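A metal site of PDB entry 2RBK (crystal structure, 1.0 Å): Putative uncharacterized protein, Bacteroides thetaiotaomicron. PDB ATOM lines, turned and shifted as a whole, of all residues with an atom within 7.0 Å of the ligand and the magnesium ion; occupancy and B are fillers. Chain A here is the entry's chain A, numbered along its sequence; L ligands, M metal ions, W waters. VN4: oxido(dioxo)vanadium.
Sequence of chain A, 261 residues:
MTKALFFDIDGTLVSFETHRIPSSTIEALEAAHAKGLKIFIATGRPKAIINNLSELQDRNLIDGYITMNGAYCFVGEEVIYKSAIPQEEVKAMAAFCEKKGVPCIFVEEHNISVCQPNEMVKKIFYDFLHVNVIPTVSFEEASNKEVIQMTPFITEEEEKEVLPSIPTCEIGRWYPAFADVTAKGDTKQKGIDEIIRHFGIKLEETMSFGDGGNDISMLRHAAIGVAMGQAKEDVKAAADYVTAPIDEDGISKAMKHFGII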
ATOM      1  N   PHE A   7      20.360  -8.980   5.295  1.00  0.00           N
ATOM      2  CA  PHE A   7      21.687  -9.536   5.570  1.00  0.00           C
ATOM      3  C   PHE A   7      22.612  -9.352   4.363  1.00  0.00           C
ATOM      4  O   PHE A   7      22.354  -9.888   3.282  1.00  0.00           O
ATOM      5  CB  PHE A   7      21.615 -11.011   5.842  1.00  0.00           C
ATOM      6  CG  PHE A   7      20.879 -11.372   7.100  1.00  0.00           C
ATOM      7  CD1 PHE A   7      19.563 -11.756   7.083  1.00  0.00           C
ATOM      8  CD2 PHE A   7      21.518 -11.315   8.338  1.00  0.00           C
ATOM      9  CE1 PHE A   7      18.890 -12.102   8.238  1.00  0.00           C
ATOM     10  CE2 PHE A   7      20.831 -11.643   9.499  1.00  0.00           C
ATOM     11  CZ  PHE A   7      19.520 -12.041   9.454  1.00  0.00           C
ATOM     12  N   ASP A   8      23.750  -8.684   4.600  1.00  0.00           N
ATOM     13  CA  ASP A   8      24.886  -8.857   3.715  1.00  0.00           C
ATOM     14  C   ASP A   8      25.320 -10.314   3.714  1.00  0.00           C
ATOM     15  O   ASP A   8      25.064 -11.050   4.662  1.00  0.00           O
ATOM     16  CB  ASP A   8      26.020  -7.970   4.210  1.00  0.00           C
ATOM     17  CG  ASP A   8      27.282  -8.089   3.447  1.00  0.00           C
ATOM     18  OD1 ASP A   8      28.344  -8.272   4.084  1.00  0.00           O
ATOM     19  OD2 ASP A   8      27.231  -7.982   2.188  1.00  0.00           O
ATOM     20  N   ILE A   9      25.988 -10.736   2.634  1.00  0.00           N
ATOM     21  CA  ILE A   9      26.469 -12.119   2.576  1.00  0.00           C
ATOM     22  C   ILE A   9      27.919 -12.171   3.116  1.00  0.00           C
ATOM     23  O   ILE A   9      28.170 -12.763   4.176  1.00  0.00           O
ATOM     24  CB  ILE A   9      26.429 -12.757   1.174  1.00  0.00           C
ATOM     25  CG1 ILE A   9      25.018 -12.750   0.607  1.00  0.00           C
ATOM     26  CG2 ILE A   9      27.028 -14.122   1.230  1.00  0.00           C
ATOM     27  CD1 ILE A   9      24.983 -13.171  -0.859  1.00  0.00           C
ATOM     28  N   ASP A  10      28.855 -11.622   2.378  1.00  0.00           N
ATOM     29  CA  ASP A  10      30.280 -11.893   2.668  1.00  0.00           C
ATOM     30  C   ASP A  10      30.736 -11.175   3.928  1.00  0.00           C
ATOM     31  O   ASP A  10      30.667  -9.964   4.037  1.00  0.00           O
ATOM     32  CB  ASP A  10      31.099 -11.520   1.465  1.00  0.00           C
ATOM     33  CG  ASP A  10      30.712 -12.332   0.265  1.00  0.00           C
ATOM     34  OD1 ASP A  10      31.005 -13.536   0.287  1.00  0.00           O
ATOM     35  OD2 ASP A  10      30.055 -11.776  -0.648  1.00  0.00           O
ATOM     36  N   GLY A  11      31.195 -11.915   4.913  1.00  0.00           N
ATOM     37  CA  GLY A  11      31.608 -11.410   6.200  1.00  0.00           C
ATOM     38  C   GLY A  11      30.470 -11.200   7.166  1.00  0.00           C
ATOM     39  O   GLY A  11      30.720 -10.753   8.298  1.00  0.00           O
ATOM     40  N   THR A  12      29.245 -11.520   6.769  1.00  0.00           N
ATOM     41  CA  THR A  12      28.047 -11.285   7.603  1.00  0.00           C
ATOM     42  C   THR A  12      27.293 -12.597   7.786  1.00  0.00           C
ATOM     43  O   THR A  12      27.117 -13.041   8.932  1.00  0.00           O
ATOM     44  CB  THR A  12      27.213 -10.166   6.950  1.00  0.00           C
ATOM     45  OG1 THR A  12      27.985  -8.968   6.928  1.00  0.00           O
ATOM     46  CG2 THR A  12      25.929  -9.938   7.790  1.00  0.00           C
ATOM     47  N   PHE A  16      34.660 -15.208   5.872  1.00  0.00           N
ATOM     48  CA  PHE A  16      35.784 -15.122   4.952  1.00  0.00           C
ATOM     49  C   PHE A  16      36.843 -16.145   5.353  1.00  0.00           C
ATOM     50  O   PHE A  16      37.641 -16.561   4.520  1.00  0.00           O
ATOM     51  CB  PHE A  16      36.410 -13.732   4.962  1.00  0.00           C
ATOM     52  CG  PHE A  16      35.673 -12.707   4.187  1.00  0.00           C
ATOM     53  CD1 PHE A  16      35.629 -12.741   2.819  1.00  0.00           C
ATOM     54  CD2 PHE A  16      34.997 -11.639   4.810  1.00  0.00           C
ATOM     55  CE1 PHE A  16      34.964 -11.744   2.078  1.00  0.00           C
ATOM     56  CE2 PHE A  16      34.387 -10.705   4.036  1.00  0.00           C
ATOM     57  CZ  PHE A  16      34.312 -10.703   2.680  1.00  0.00           C
ATOM     58  N   ILE A  41      18.316 -11.003   1.514  1.00  0.00           N
ATOM     59  CA  ILE A  41      19.730 -10.850   1.177  1.00  0.00           C
ATOM     60  C   ILE A  41      19.977  -9.476   0.637  1.00  0.00           C
ATOM     61  O   ILE A  41      19.148  -8.995  -0.149  1.00  0.00           O
ATOM     62  CB  ILE A  41      20.131 -11.942   0.178  1.00  0.00           C
ATOM     63  CG1 ILE A  41      19.947 -13.347   0.789  1.00  0.00           C
ATOM     64  CG2 ILE A  41      21.532 -11.742  -0.367  1.00  0.00           C
ATOM     65  CD1 ILE A  41      20.760 -13.588   2.025  1.00  0.00           C
ATOM     66  N   ALA A  42      21.062  -8.822   1.035  1.00  0.00           N
ATOM     67  CA  ALA A  42      21.427  -7.499   0.531  1.00  0.00           C
ATOM     68  C   ALA A  42      22.911  -7.556   0.249  1.00  0.00           C
ATOM     69  O   ALA A  42      23.732  -7.382   1.153  1.00  0.00           O
ATOM     70  CB  ALA A  42      21.023  -6.408   1.477  1.00  0.00           C
ATOM     71  N   THR A  43      23.279  -7.753  -1.047  1.00  0.00           N
ATOM     72  CA  THR A  43      24.641  -8.052  -1.440  1.00  0.00           C
ATOM     73  C   THR A  43      25.069  -7.223  -2.630  1.00  0.00           C
ATOM     74  O   THR A  43      24.301  -6.852  -3.497  1.00  0.00           O
ATOM     75  CB  THR A  43      24.778  -9.566  -1.704  1.00  0.00           C
ATOM     76  OG1 THR A  43      26.121  -9.908  -2.028  1.00  0.00           O
ATOM     77  CG2 THR A  43      23.919 -10.030  -2.875  1.00  0.00           C
ATOM     78  N   GLY A  44      26.410  -6.984  -2.694  1.00  0.00           N
ATOM     79  CA  GLY A  44      27.059  -6.526  -3.866  1.00  0.00           C
ATOM     80  C   GLY A  44      27.170  -7.561  -4.945  1.00  0.00           C
ATOM     81  O   GLY A  44      27.382  -7.270  -6.133  1.00  0.00           O
ATOM     82  N   ARG A  45      27.074  -8.855  -4.613  1.00  0.00           N
ATOM     83  CA  ARG A  45      27.172  -9.871  -5.632  1.00  0.00           C
ATOM     84  C   ARG A  45      25.975  -9.806  -6.568  1.00  0.00           C
ATOM     85  O   ARG A  45      24.836  -9.636  -6.120  1.00  0.00           O
ATOM     86  CB  ARG A  45      27.193 -11.262  -5.012  1.00  0.00           C
ATOM     87  CG  ARG A  45      28.385 -11.632  -4.206  1.00  0.00           C
ATOM     88  CD  ARG A  45      28.316 -13.027  -3.651  1.00  0.00           C
ATOM     89  NE  ARG A  45      29.508 -13.380  -2.883  1.00  0.00           N
ATOM     90  CZ  ARG A  45      30.315 -14.405  -3.124  1.00  0.00           C
ATOM     91  NH1 ARG A  45      30.117 -15.241  -4.155  1.00  0.00           N
ATOM     92  NH2 ARG A  45      31.349 -14.567  -2.305  1.00  0.00           N
ATOM     93  N   ASN A  52      26.977 -19.375  -2.576  1.00  0.00           N
ATOM     94  CA  ASN A  52      27.433 -19.665  -1.196  1.00  0.00           C
ATOM     95  C   ASN A  52      26.290 -19.647  -0.206  1.00  0.00           C
ATOM     96  O   ASN A  52      26.536 -19.673   1.003  1.00  0.00           O
ATOM     97  CB  ASN A  52      28.567 -18.700  -0.854  1.00  0.00           C
ATOM     98  CG  ASN A  52      28.208 -17.236  -0.918  1.00  0.00           C
ATOM     99  OD1 ASN A  52      27.073 -16.888  -1.357  1.00  0.00           O
ATOM    100  ND2 ASN A  52      29.177 -16.394  -0.575  1.00  0.00           N
ATOM    101  N   ASN A  69      24.195  -4.380  -5.115  1.00  0.00           N
ATOM    102  CA  ASN A  69      24.162  -3.167  -4.297  1.00  0.00           C
ATOM    103  C   ASN A  69      22.876  -2.382  -4.463  1.00  0.00           C
ATOM    104  O   ASN A  69      22.862  -1.167  -4.309  1.00  0.00           O
ATOM    105  CB  ASN A  69      25.370  -2.240  -4.575  1.00  0.00           C
ATOM    106  CG  ASN A  69      26.639  -2.854  -4.089  1.00  0.00           C
ATOM    107  OD1 ASN A  69      26.876  -2.902  -2.884  1.00  0.00           O
ATOM    108  ND2 ASN A  69      27.443  -3.406  -4.993  1.00  0.00           N
ATOM    109  N   ARG A 173      32.628  -0.513  -1.566  1.00  0.00           N
ATOM    110  CA  ARG A 173      33.474  -1.747  -1.415  1.00  0.00           C
ATOM    111  C   ARG A 173      33.002  -2.674  -0.270  1.00  0.00           C
ATOM    112  O   ARG A 173      32.609  -2.256   0.821  1.00  0.00           O
ATOM    113  CB  ARG A 173      34.916  -1.468  -1.125  1.00  0.00           C
ATOM    114  CG  ARG A 173      35.662  -0.515  -1.989  1.00  0.00           C
ATOM    115  CD  ARG A 173      37.168  -0.302  -1.805  1.00  0.00           C
ATOM    116  NE  ARG A 173      37.565   0.681  -2.846  1.00  0.00           N
ATOM    117  CZ  ARG A 173      38.396   0.433  -3.789  1.00  0.00           C
ATOM    118  NH1 ARG A 173      39.048  -0.724  -3.817  1.00  0.00           N
ATOM    119  NH2 ARG A 173      38.679   1.330  -4.740  1.00  0.00           N
ATOM    120  N   TRP A 174      33.059  -4.008  -0.535  1.00  0.00           N
ATOM    121  CA  TRP A 174      32.940  -5.064   0.416  1.00  0.00           C
ATOM    122  C   TRP A 174      34.158  -5.914   0.673  1.00  0.00           C
ATOM    123  O   TRP A 174      34.219  -6.716   1.523  1.00  0.00           O
ATOM    124  CB  TRP A 174      31.757  -5.993   0.075  1.00  0.00           C
ATOM    125  CG  TRP A 174      31.674  -6.607  -1.274  1.00  0.00           C
ATOM    126  CD1 TRP A 174      31.145  -6.039  -2.435  1.00  0.00           C
ATOM    127  CD2 TRP A 174      32.088  -7.927  -1.663  1.00  0.00           C
ATOM    128  NE1 TRP A 174      31.211  -6.888  -3.457  1.00  0.00           N
ATOM    129  CE2 TRP A 174      31.769  -8.059  -3.043  1.00  0.00           C
ATOM    130  CE3 TRP A 174      32.663  -9.005  -1.006  1.00  0.00           C
ATOM    131  CZ2 TRP A 174      32.002  -9.211  -3.804  1.00  0.00           C
ATOM    132  CZ3 TRP A 174      32.909 -10.157  -1.732  1.00  0.00           C
ATOM    133  CH2 TRP A 174      32.576 -10.243  -3.070  1.00  0.00           C
ATOM    134  N   TYR A 175      35.173  -5.613  -0.141  1.00  0.00           N
ATOM    135  CA  TYR A 175      36.442  -6.287  -0.041  1.00  0.00           C
ATOM    136  C   TYR A 175      37.541  -5.302  -0.486  1.00  0.00           C
ATOM    137  O   TYR A 175      37.197  -4.542  -1.429  1.00  0.00           O
ATOM    138  CB  TYR A 175      36.487  -7.580  -0.881  1.00  0.00           C
ATOM    139  CG  TYR A 175      37.643  -8.478  -0.618  1.00  0.00           C
ATOM    140  CD1 TYR A 175      37.608  -9.355   0.484  1.00  0.00           C
ATOM    141  CD2 TYR A 175      38.783  -8.475  -1.411  1.00  0.00           C
ATOM    142  CE1 TYR A 175      38.664 -10.197   0.758  1.00  0.00           C
ATOM    143  CE2 TYR A 175      39.833  -9.308  -1.146  1.00  0.00           C
ATOM    144  CZ  TYR A 175      39.762 -10.171  -0.062  1.00  0.00           C
ATOM    145  OH  TYR A 175      40.840 -10.978   0.177  1.00  0.00           O
ATOM    146  N   ASP A 180      32.546  -1.889  -6.385  1.00  0.00           N
ATOM    147  CA  ASP A 180      31.369  -2.060  -7.203  1.00  0.00           C
ATOM    148  C   ASP A 180      30.797  -0.696  -7.572  1.00  0.00           C
ATOM    149  O   ASP A 180      30.600   0.153  -6.682  1.00  0.00           O
ATOM    150  CB  ASP A 180      30.277  -2.835  -6.460  1.00  0.00           C
ATOM    151  CG  ASP A 180      30.603  -4.290  -6.170  1.00  0.00           C
ATOM    152  OD1 ASP A 180      31.298  -4.945  -6.971  1.00  0.00           O
ATOM    153  OD2 ASP A 180      30.076  -4.738  -5.102  1.00  0.00           O
ATOM    154  N   LYS A 188      22.573  -0.339  -1.175  1.00  0.00           N
ATOM    155  CA  LYS A 188      21.670  -1.265  -0.475  1.00  0.00           C
ATOM    156  C   LYS A 188      20.497  -0.559   0.189  1.00  0.00           C
ATOM    157  O   LYS A 188      19.458  -1.199   0.406  1.00  0.00           O
ATOM    158  CB  LYS A 188      22.466  -2.119   0.494  1.00  0.00           C
ATOM    159  CG  LYS A 188      23.429  -3.076  -0.156  1.00  0.00           C
ATOM    160  CD  LYS A 188      24.255  -3.831   0.823  1.00  0.00           C
ATOM    161  CE  LYS A 188      25.353  -4.644   0.126  1.00  0.00           C
ATOM    162  NZ  LYS A 188      26.049  -5.582   1.047  1.00  0.00           N
ATOM    163  N   GLY A 210      25.652  -6.024   8.603  1.00  0.00           N
ATOM    164  CA  GLY A 210      26.748  -5.907   7.633  1.00  0.00           C
ATOM    165  C   GLY A 210      28.081  -5.795   8.292  1.00  0.00           C
ATOM    166  O   GLY A 210      28.224  -5.599   9.500  1.00  0.00           O
ATOM    167  N   ASP A 211      29.118  -5.938   7.435  1.00  0.00           N
ATOM    168  CA  ASP A 211      30.490  -5.898   7.856  1.00  0.00           C
ATOM    169  C   ASP A 211      31.330  -4.923   7.049  1.00  0.00           C
ATOM    170  O   ASP A 211      32.510  -4.817   7.420  1.00  0.00           O
ATOM    171  CB  ASP A 211      31.207  -7.272   7.738  1.00  0.00           C
ATOM    172  CG  ASP A 211      31.483  -7.630   6.302  1.00  0.00           C
ATOM    173  OD1 ASP A 211      30.549  -7.448   5.492  1.00  0.00           O
ATOM    174  OD2 ASP A 211      32.635  -8.040   5.983  1.00  0.00           O
ATOM    175  N   GLY A 212      30.825  -4.291   6.022  1.00  0.00           N
ATOM    176  CA  GLY A 212      31.689  -3.605   5.038  1.00  0.00           C
ATOM    177  C   GLY A 212      31.230  -2.207   4.715  1.00  0.00           C
ATOM    178  O   GLY A 212      30.119  -1.793   5.043  1.00  0.00           O
ATOM    179  N   GLY A 213      32.116  -1.477   4.021  1.00  0.00           N
ATOM    180  CA  GLY A 213      31.790  -0.126   3.650  1.00  0.00           C
ATOM    181  C   GLY A 213      30.532  -0.019   2.796  1.00  0.00           C
ATOM    182  O   GLY A 213      29.820   0.989   2.959  1.00  0.00           O
ATOM    183  N   ASN A 214      30.242  -0.993   1.953  1.00  0.00           N
ATOM    184  CA  ASN A 214      29.055  -0.936   1.134  1.00  0.00           C
ATOM    185  C   ASN A 214      27.761  -1.264   1.888  1.00  0.00           C
ATOM    186  O   ASN A 214      26.705  -1.255   1.296  1.00  0.00           O
ATOM    187  CB  ASN A 214      29.154  -1.816  -0.114  1.00  0.00           C
ATOM    188  CG  ASN A 214      29.120  -3.328   0.152  1.00  0.00           C
ATOM    189  OD1 ASN A 214      29.563  -3.721   1.244  1.00  0.00           O
ATOM    190  ND2 ASN A 214      28.697  -4.154  -0.797  1.00  0.00           N
ATOM    191  N   ASP A 215      27.893  -1.518   3.223  1.00  0.00           N
ATOM    192  CA  ASP A 215      26.770  -1.700   4.082  1.00  0.00           C
ATOM    193  C   ASP A 215      26.429  -0.438   4.868  1.00  0.00           C
ATOM    194  O   ASP A 215      25.393  -0.405   5.530  1.00  0.00           O
ATOM    195  CB  ASP A 215      27.046  -2.829   5.093  1.00  0.00           C
ATOM    196  CG  ASP A 215      27.325  -4.142   4.407  1.00  0.00           C
ATOM    197  OD1 ASP A 215      26.522  -4.434   3.454  1.00  0.00           O
ATOM    198  OD2 ASP A 215      28.236  -4.868   4.825  1.00  0.00           O
HETATM  199  V   VN4 L   1      28.372  -8.457   0.580  1.00  0.00           V
HETATM  200  O1  VN4 L   1      27.536  -9.869   0.338  1.00  0.00           O
HETATM  201  O2  VN4 L   1      29.827  -8.418   1.556  1.00  0.00           O
HETATM  202  O3  VN4 L   1      28.313  -7.002  -0.553  1.00  0.00           O
HETATM  203 MG    MG M   1      30.299  -7.980   3.514  1.00  0.00          MG
HETATM  204  O   HOH W   1      29.366  -9.199  -1.136  1.00  0.00           O
HETATM  205  O   HOH W   2      29.886  -5.957   3.124  1.00  0.00           O
HETATM  206  O   HOH W   3      32.356  -7.814   3.255  1.00  0.00           O
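V of the ligand is bound by OD2 of Asp 8 (2.0 Å).
OD1 of Asp 8 sits close to OG1 of Thr 12, 2.9 Å away.
OD2 of Asp 215 lies within hydrogen-bond range of N of Asp 211, 3.0 Å away.
N of Asp 211 sits at hydrogen-bond distance from OG1 of Thr 12 (3.3 Å).
The side-chain hydroxyl (OG1) of Thr 43 is in hydrogen-bond range of the backbone NH (N) of Arg 45, 2.9 Å away.
The side-chain amide oxygen (OD1) of Asn 69 sits at hydrogen-bond distance from the side-chain amide nitrogen (ND2) of Asn 214 (3.0 Å).
NZ of Lys 188 lies within salt-bridge range of OD1 of Asp 215 (2.7 Å).
The backbone carbonyl oxygen (O) of Ala 42 lies within hydrogen-bond range of the side-chain amino group (NZ) of Lys 188 (2.9 Å).
O of Asn 69 sits at hydrogen-bond distance from N of Lys 188, 3.3 Å away.
The backbone NH (N) of Ile 9 lies close to an oxygen (O1) of the ligand.
The side-chain hydroxyl of Thr 43 sits close to an oxygen (O1) of the ligand.
The backbone NH (N) of Gly 44 sits close to an oxygen (O3) of the ligand.
The side-chain amino group (NZ) of Lys 188 lies close to an oxygen (O3) of the ligand (3.1 Å).
ND2 of Asn 214 sits close to O3 of the ligand.
Merely in contact with the ligand: Trp 174 (3.4 Å).
Within 4 Å of the ligand: Asp 8, Ile 9, Asp 10, Thr 43, Gly 44, Trp 174, Lys 188 and Asn 214.
The nearest printed residue that does not touch the ligand is Asp 211 (4.1 Å).
OD2 of Asp 215 touches the magnesium ion, 3.96 Å away.
Four residues have an atom within 4 Å of the magnesium ion: Asp 8, Asp 10, Asp 211 and Asp 215.
The magnesium ion is bound by OD1 of Asp 8, O2 of the ligand, OD1 of Asp 211, water W3, O of Asp 10 and water W2.
Water W2 lies within hydrogen-bond range of OD2 of Asp 215, OD1 of Asn 214 and N of Gly 212.
Water W3 bridges OD2 of Asp 211 (2.8 Å) and O of Trp 174 (2.8 Å).
Water W1 lies within hydrogen-bond range of the side-chain carboxylate of Asp 10 and the side-chain hydroxyl of Thr 43.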
